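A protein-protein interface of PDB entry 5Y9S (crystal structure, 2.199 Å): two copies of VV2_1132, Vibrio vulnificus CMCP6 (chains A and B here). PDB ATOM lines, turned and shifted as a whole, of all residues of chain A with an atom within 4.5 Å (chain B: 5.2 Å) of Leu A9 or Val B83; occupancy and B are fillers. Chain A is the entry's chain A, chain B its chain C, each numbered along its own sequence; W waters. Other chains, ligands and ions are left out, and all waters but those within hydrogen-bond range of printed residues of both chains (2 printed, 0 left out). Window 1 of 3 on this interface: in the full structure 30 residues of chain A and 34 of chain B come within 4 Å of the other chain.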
ATOM      1  N   ASN A   7      19.034 -17.899  12.244  1.00  0.00           N
ATOM      2  CA  ASN A   7      18.752 -16.524  11.814  1.00  0.00           C
ATOM      3  C   ASN A   7      19.585 -15.508  12.610  1.00  0.00           C
ATOM      4  O   ASN A   7      19.059 -14.715  13.395  1.00  0.00           O
ATOM      5  CB  ASN A   7      17.251 -16.258  11.954  1.00  0.00           C
ATOM      6  CG  ASN A   7      16.838 -14.930  11.386  1.00  0.00           C
ATOM      7  OD1 ASN A   7      17.600 -14.296  10.648  1.00  0.00           O
ATOM      8  ND2 ASN A   7      15.626 -14.485  11.734  1.00  0.00           N
ATOM      9  N   PRO A   8      20.899 -15.506  12.426  1.00  0.00           N
ATOM     10  CA  PRO A   8      21.741 -14.645  13.253  1.00  0.00           C
ATOM     11  C   PRO A   8      21.620 -13.181  12.858  1.00  0.00           C
ATOM     12  O   PRO A   8      21.404 -12.833  11.694  1.00  0.00           O
ATOM     13  CB  PRO A   8      23.151 -15.171  12.978  1.00  0.00           C
ATOM     14  CG  PRO A   8      23.074 -15.692  11.593  1.00  0.00           C
ATOM     15  CD  PRO A   8      21.695 -16.293  11.467  1.00  0.00           C
ATOM     16  N   LEU A   9      21.738 -12.319  13.854  1.00  0.00           N
ATOM     17  CA  LEU A   9      22.034 -10.922  13.579  1.00  0.00           C
ATOM     18  C   LEU A   9      23.425 -10.817  12.965  1.00  0.00           C
ATOM     19  O   LEU A   9      24.375 -11.443  13.438  1.00  0.00           O
ATOM     20  CB  LEU A   9      21.957 -10.093  14.864  1.00  0.00           C
ATOM     21  CG  LEU A   9      22.431  -8.632  14.766  1.00  0.00           C
ATOM     22  CD1 LEU A   9      21.496  -7.830  13.912  1.00  0.00           C
ATOM     23  CD2 LEU A   9      22.501  -7.973  16.130  1.00  0.00           C
ATOM     24  N   GLU A  10      23.550 -10.040  11.904  1.00  0.00           N
ATOM     25  CA  GLU A  10      24.841  -9.852  11.271  1.00  0.00           C
ATOM     26  C   GLU A  10      25.311  -8.434  11.545  1.00  0.00           C
ATOM     27  O   GLU A  10      24.615  -7.466  11.221  1.00  0.00           O
ATOM     28  CB  GLU A  10      24.765 -10.157   9.779  1.00  0.00           C
ATOM     29  CG  GLU A  10      24.239 -11.539   9.537  1.00  0.00           C
ATOM     30  CD  GLU A  10      24.473 -11.980   8.126  1.00  0.00           C
ATOM     31  OE1 GLU A  10      23.847 -12.961   7.690  1.00  0.00           O
ATOM     32  OE2 GLU A  10      25.282 -11.327   7.450  1.00  0.00           O
ATOM     33  N   PHE A  11      26.487  -8.338  12.166  1.00  0.00           N
ATOM     34  CA  PHE A  11      27.068  -7.077  12.603  1.00  0.00           C
ATOM     35  C   PHE A  11      27.004  -6.017  11.513  1.00  0.00           C
ATOM     36  O   PHE A  11      26.658  -4.864  11.783  1.00  0.00           O
ATOM     37  CB  PHE A  11      28.509  -7.359  13.050  1.00  0.00           C
ATOM     38  CG  PHE A  11      29.371  -6.140  13.212  1.00  0.00           C
ATOM     39  CD1 PHE A  11      30.034  -5.581  12.118  1.00  0.00           C
ATOM     40  CD2 PHE A  11      29.572  -5.582  14.468  1.00  0.00           C
ATOM     41  CE1 PHE A  11      30.836  -4.461  12.264  1.00  0.00           C
ATOM     42  CE2 PHE A  11      30.397  -4.461  14.627  1.00  0.00           C
ATOM     43  CZ  PHE A  11      31.021  -3.900  13.522  1.00  0.00           C
ATOM     44  N   TRP A  13      24.983  -5.347   9.192  1.00  0.00           N
ATOM     45  CA  TRP A  13      23.688  -4.721   8.991  1.00  0.00           C
ATOM     46  C   TRP A  13      23.569  -3.451   9.811  1.00  0.00           C
ATOM     47  O   TRP A  13      22.866  -2.514   9.416  1.00  0.00           O
ATOM     48  CB  TRP A  13      22.581  -5.657   9.422  1.00  0.00           C
ATOM     49  CG  TRP A  13      22.402  -6.916   8.635  1.00  0.00           C
ATOM     50  CD1 TRP A  13      22.877  -7.203   7.385  1.00  0.00           C
ATOM     51  CD2 TRP A  13      21.639  -8.048   9.051  1.00  0.00           C
ATOM     52  NE1 TRP A  13      22.467  -8.458   7.010  1.00  0.00           N
ATOM     53  CE2 TRP A  13      21.718  -9.008   8.020  1.00  0.00           C
ATOM     54  CE3 TRP A  13      20.894  -8.347  10.201  1.00  0.00           C
ATOM     55  CZ2 TRP A  13      21.061 -10.261   8.093  1.00  0.00           C
ATOM     56  CZ3 TRP A  13      20.264  -9.621  10.290  1.00  0.00           C
ATOM     57  CH2 TRP A  13      20.357 -10.548   9.230  1.00  0.00           C
ATOM     58  N   TRP A  50      14.765  -9.575  10.008  1.00  0.00           N
ATOM     59  CA  TRP A  50      15.260 -10.073  11.299  1.00  0.00           C
ATOM     60  C   TRP A  50      14.576  -9.368  12.460  1.00  0.00           C
ATOM     61  O   TRP A  50      14.140 -10.006  13.429  1.00  0.00           O
ATOM     62  CB  TRP A  50      16.783  -9.871  11.396  1.00  0.00           C
ATOM     63  CG  TRP A  50      17.388 -10.350  12.695  1.00  0.00           C
ATOM     64  CD1 TRP A  50      17.868 -11.601  12.963  1.00  0.00           C
ATOM     65  CD2 TRP A  50      17.582  -9.580  13.905  1.00  0.00           C
ATOM     66  NE1 TRP A  50      18.334 -11.658  14.265  1.00  0.00           N
ATOM     67  CE2 TRP A  50      18.176 -10.436  14.858  1.00  0.00           C
ATOM     68  CE3 TRP A  50      17.334  -8.254  14.260  1.00  0.00           C
ATOM     69  CZ2 TRP A  50      18.515 -10.006  16.146  1.00  0.00           C
ATOM     70  CZ3 TRP A  50      17.663  -7.832  15.552  1.00  0.00           C
ATOM     71  CH2 TRP A  50      18.238  -8.708  16.473  1.00  0.00           C
ATOM     72  N   LEU A  79      25.140  -1.523  20.269  1.00  0.00           N
ATOM     73  CA  LEU A  79      25.778  -2.756  19.823  1.00  0.00           C
ATOM     74  C   LEU A  79      27.148  -2.470  19.218  1.00  0.00           C
ATOM     75  O   LEU A  79      28.162  -3.013  19.669  1.00  0.00           O
ATOM     76  CB  LEU A  79      24.881  -3.493  18.830  1.00  0.00           C
ATOM     77  CG  LEU A  79      23.918  -4.381  19.603  1.00  0.00           C
ATOM     78  CD1 LEU A  79      22.831  -4.984  18.698  1.00  0.00           C
ATOM     79  CD2 LEU A  79      24.736  -5.456  20.322  1.00  0.00           C
ATOM     80  N   PHE B  11      27.942 -13.421  15.973  1.00  0.00           N
ATOM     81  CA  PHE B  11      27.428 -13.593  17.327  1.00  0.00           C
ATOM     82  C   PHE B  11      27.355 -15.069  17.754  1.00  0.00           C
ATOM     83  O   PHE B  11      27.420 -15.343  18.957  1.00  0.00           O
ATOM     84  CB  PHE B  11      26.091 -12.849  17.416  1.00  0.00           C
ATOM     85  CG  PHE B  11      26.249 -11.341  17.378  1.00  0.00           C
ATOM     86  CD1 PHE B  11      26.884 -10.679  18.423  1.00  0.00           C
ATOM     87  CD2 PHE B  11      25.842 -10.592  16.280  1.00  0.00           C
ATOM     88  CE1 PHE B  11      27.061  -9.290  18.399  1.00  0.00           C
ATOM     89  CE2 PHE B  11      26.036  -9.195  16.247  1.00  0.00           C
ATOM     90  CZ  PHE B  11      26.641  -8.549  17.307  1.00  0.00           C
ATOM     91  N   LEU B  79      27.180  -8.548  25.096  1.00  0.00           N
ATOM     92  CA  LEU B  79      26.695  -8.490  23.728  1.00  0.00           C
ATOM     93  C   LEU B  79      25.495  -9.399  23.545  1.00  0.00           C
ATOM     94  O   LEU B  79      24.485  -8.992  22.964  1.00  0.00           O
ATOM     95  CB  LEU B  79      27.807  -8.884  22.747  1.00  0.00           C
ATOM     96  CG  LEU B  79      28.944  -7.875  22.638  1.00  0.00           C
ATOM     97  CD1 LEU B  79      30.168  -8.505  21.954  1.00  0.00           C
ATOM     98  CD2 LEU B  79      28.448  -6.653  21.878  1.00  0.00           C
ATOM     99  N   LEU B  80      25.592 -10.646  24.022  1.00  0.00           N
ATOM    100  CA  LEU B  80      24.500 -11.588  23.789  1.00  0.00           C
ATOM    101  C   LEU B  80      23.199 -11.055  24.349  1.00  0.00           C
ATOM    102  O   LEU B  80      22.138 -11.224  23.743  1.00  0.00           O
ATOM    103  CB  LEU B  80      24.798 -12.946  24.411  1.00  0.00           C
ATOM    104  CG  LEU B  80      25.321 -13.955  23.394  1.00  0.00           C
ATOM    105  CD1 LEU B  80      25.903 -15.163  24.103  1.00  0.00           C
ATOM    106  CD2 LEU B  80      24.222 -14.364  22.423  1.00  0.00           C
ATOM    107  N   ASN B  81      23.263 -10.412  25.514  1.00  0.00           N
ATOM    108  CA  ASN B  81      22.065  -9.822  26.085  1.00  0.00           C
ATOM    109  C   ASN B  81      21.594  -8.608  25.291  1.00  0.00           C
ATOM    110  O   ASN B  81      20.386  -8.361  25.220  1.00  0.00           O
ATOM    111  CB  ASN B  81      22.309  -9.424  27.531  1.00  0.00           C
ATOM    112  CG  ASN B  81      21.053  -8.901  28.195  1.00  0.00           C
ATOM    113  OD1 ASN B  81      20.126  -9.664  28.472  1.00  0.00           O
ATOM    114  ND2 ASN B  81      21.015  -7.594  28.458  1.00  0.00           N
ATOM    115  N   GLN B  82      22.518  -7.821  24.717  1.00  0.00           N
ATOM    116  CA  GLN B  82      22.079  -6.670  23.936  1.00  0.00           C
ATOM    117  C   GLN B  82      21.317  -7.128  22.702  1.00  0.00           C
ATOM    118  O   GLN B  82      20.317  -6.506  22.324  1.00  0.00           O
ATOM    119  CB  GLN B  82      23.258  -5.774  23.536  1.00  0.00           C
ATOM    120  CG  GLN B  82      23.886  -4.985  24.683  1.00  0.00           C
ATOM    121  CD  GLN B  82      24.795  -3.851  24.218  1.00  0.00           C
ATOM    122  OE1 GLN B  82      24.495  -3.153  23.237  1.00  0.00           O
ATOM    123  NE2 GLN B  82      25.917  -3.670  24.906  1.00  0.00           N
ATOM    124  N   VAL B  83      21.759  -8.222  22.072  1.00  0.00           N
ATOM    125  CA  VAL B  83      21.050  -8.729  20.898  1.00  0.00           C
ATOM    126  C   VAL B  83      19.683  -9.255  21.298  1.00  0.00           C
ATOM    127  O   VAL B  83      18.678  -8.987  20.635  1.00  0.00           O
ATOM    128  CB  VAL B  83      21.868  -9.818  20.195  1.00  0.00           C
ATOM    129  CG1 VAL B  83      21.025 -10.468  19.094  1.00  0.00           C
ATOM    130  CG2 VAL B  83      23.172  -9.239  19.627  1.00  0.00           C
ATOM    131  N   LYS B  84      19.628  -9.976  22.414  1.00  0.00           N
ATOM    132  CA  LYS B  84      18.375 -10.546  22.902  1.00  0.00           C
ATOM    133  C   LYS B  84      17.362  -9.449  23.211  1.00  0.00           C
ATOM    134  O   LYS B  84      16.219  -9.485  22.740  1.00  0.00           O
ATOM    135  CB  LYS B  84      18.674 -11.407  24.137  1.00  0.00           C
ATOM    136  CG  LYS B  84      17.470 -11.875  24.949  1.00  0.00           C
ATOM    137  CD  LYS B  84      17.898 -12.492  26.294  1.00  0.00           C
ATOM    138  CE  LYS B  84      16.889 -13.526  26.798  1.00  0.00           C
ATOM    139  NZ  LYS B  84      17.514 -14.657  27.559  1.00  0.00           N
ATOM    140  N   VAL B  85      17.778  -8.455  23.995  1.00  0.00           N
ATOM    141  CA  VAL B  85      16.916  -7.332  24.352  1.00  0.00           C
ATOM    142  C   VAL B  85      16.444  -6.588  23.106  1.00  0.00           C
ATOM    143  O   VAL B  85      15.302  -6.129  23.043  1.00  0.00           O
ATOM    144  CB  VAL B  85      17.668  -6.404  25.321  1.00  0.00           C
ATOM    145  CG1 VAL B  85      17.059  -4.978  25.345  1.00  0.00           C
ATOM    146  CG2 VAL B  85      17.691  -7.032  26.713  1.00  0.00           C
ATOM    147  N   THR B  86      17.312  -6.458  22.102  1.00  0.00           N
ATOM    148  CA  THR B  86      16.916  -5.831  20.849  1.00  0.00           C
ATOM    149  C   THR B  86      15.828  -6.646  20.179  1.00  0.00           C
ATOM    150  O   THR B  86      14.806  -6.110  19.754  1.00  0.00           O
ATOM    151  CB  THR B  86      18.122  -5.698  19.911  1.00  0.00           C
ATOM    152  OG1 THR B  86      19.149  -4.913  20.530  1.00  0.00           O
ATOM    153  CG2 THR B  86      17.710  -5.058  18.601  1.00  0.00           C
ATOM    154  N   LYS B  87      16.041  -7.954  20.081  1.00  0.00           N
ATOM    155  CA  LYS B  87      15.056  -8.840  19.478  1.00  0.00           C
ATOM    156  C   LYS B  87      13.744  -8.801  20.245  1.00  0.00           C
ATOM    157  O   LYS B  87      12.665  -8.748  19.643  1.00  0.00           O
ATOM    158  CB  LYS B  87      15.602 -10.268  19.440  1.00  0.00           C
ATOM    159  CG  LYS B  87      14.725 -11.245  18.680  1.00  0.00           C
ATOM    160  CD  LYS B  87      14.994 -11.137  17.192  1.00  0.00           C
ATOM    161  CE  LYS B  87      14.677 -12.425  16.429  1.00  0.00           C
ATOM    162  NZ  LYS B  87      15.010 -12.271  14.966  1.00  0.00           N
ATOM    163  N   GLU B  88      13.816  -8.809  21.580  1.00  0.00           N
ATOM    164  CA  GLU B  88      12.594  -8.872  22.371  1.00  0.00           C
ATOM    165  C   GLU B  88      11.849  -7.549  22.315  1.00  0.00           C
ATOM    166  O   GLU B  88      10.645  -7.530  22.053  1.00  0.00           O
ATOM    167  CB  GLU B  88      12.916  -9.259  23.819  1.00  0.00           C
ATOM    168  CG  GLU B  88      13.425 -10.696  23.962  1.00  0.00           C
ATOM    169  CD  GLU B  88      13.850 -11.067  25.389  1.00  0.00           C
ATOM    170  OE1 GLU B  88      14.315 -10.179  26.150  1.00  0.00           O
ATOM    171  OE2 GLU B  88      13.723 -12.266  25.739  1.00  0.00           O
HETATM  172  O   HOH W   1      22.200  -2.443  21.737  1.00  0.00           O
HETATM  173  O   HOH W   2      17.184 -14.321  15.179  1.00  0.00           O
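The backbone carbonyl oxygen (O) of Trp A50 is in hydrogen-bond range of the side-chain amino group (NZ) of Lys B87, at 2.9 Å. OE1 of Gln B82 sits at hydrogen-bond distance from N of Leu A79 (3.4 Å).
The backbone carbonyl oxygen of Gln B82 lies within hydrogen-bond range of the side-chain hydroxyl of Thr B86. NE1 of Trp A50 sits at hydrogen-bond distance from O of Asn A7 (3.3 Å).
Among the printed residues, pairs that only touch across the chains: Asn A7 with Lys B87, Leu A9 with Phe B11, Leu A9 with Val B83 and Trp A50 with Val B83.
Leu A9 touches just these residues of chain B: Phe B11 (3.3 Å) and Val B83 (3.8 Å). Val B83 touches two residues of chain A. Of the printed residues of chain A, Lys B87 touches Asn A7 (3.97 Å) and Trp A50 (2.9 Å). Printed residues of chain B within 4 Å of Asn A7: Lys B87. Printed residues of chain B within 4 Å of Leu A79: Gln B82. Printed residues of chain A within 4 Å of Phe B11: Leu A9. Printed residues of chain A within 4 Å of Gln B82: Leu A79. The nearest residue of chain A that does not touch Val B83 is Leu A79 (4.2 Å).
Printed residues of chain B that touch a printed residue of chain A: Phe B11, Gln B82, Val B83 and Lys B87. Of the 8 printed residues of chain A, 4 touch a printed residue of chain B. Hydrophobic or aromatic side chains of chain A within 4 Å of the printed part of chain B: Leu A9, Trp A50 and Leu A79. Among the printed residues, no Asp or Glu carboxylate lies within 4 Å of a Lys or Arg side-chain nitrogen of the other chain.
Positions printed for both chains: 11 and 79.
Water W2 lies within hydrogen-bond range of O of Asn A7 (2.6 Å), NZ of Lys B87 (3.0 Å) and NE1 of Trp A50 (3.0 Å). Water W1 lies within hydrogen-bond range of the side-chain amide oxygen (OE1) of Gln B82 (2.8 Å) and the backbone NH (N) of Leu A79 (3.4 Å).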
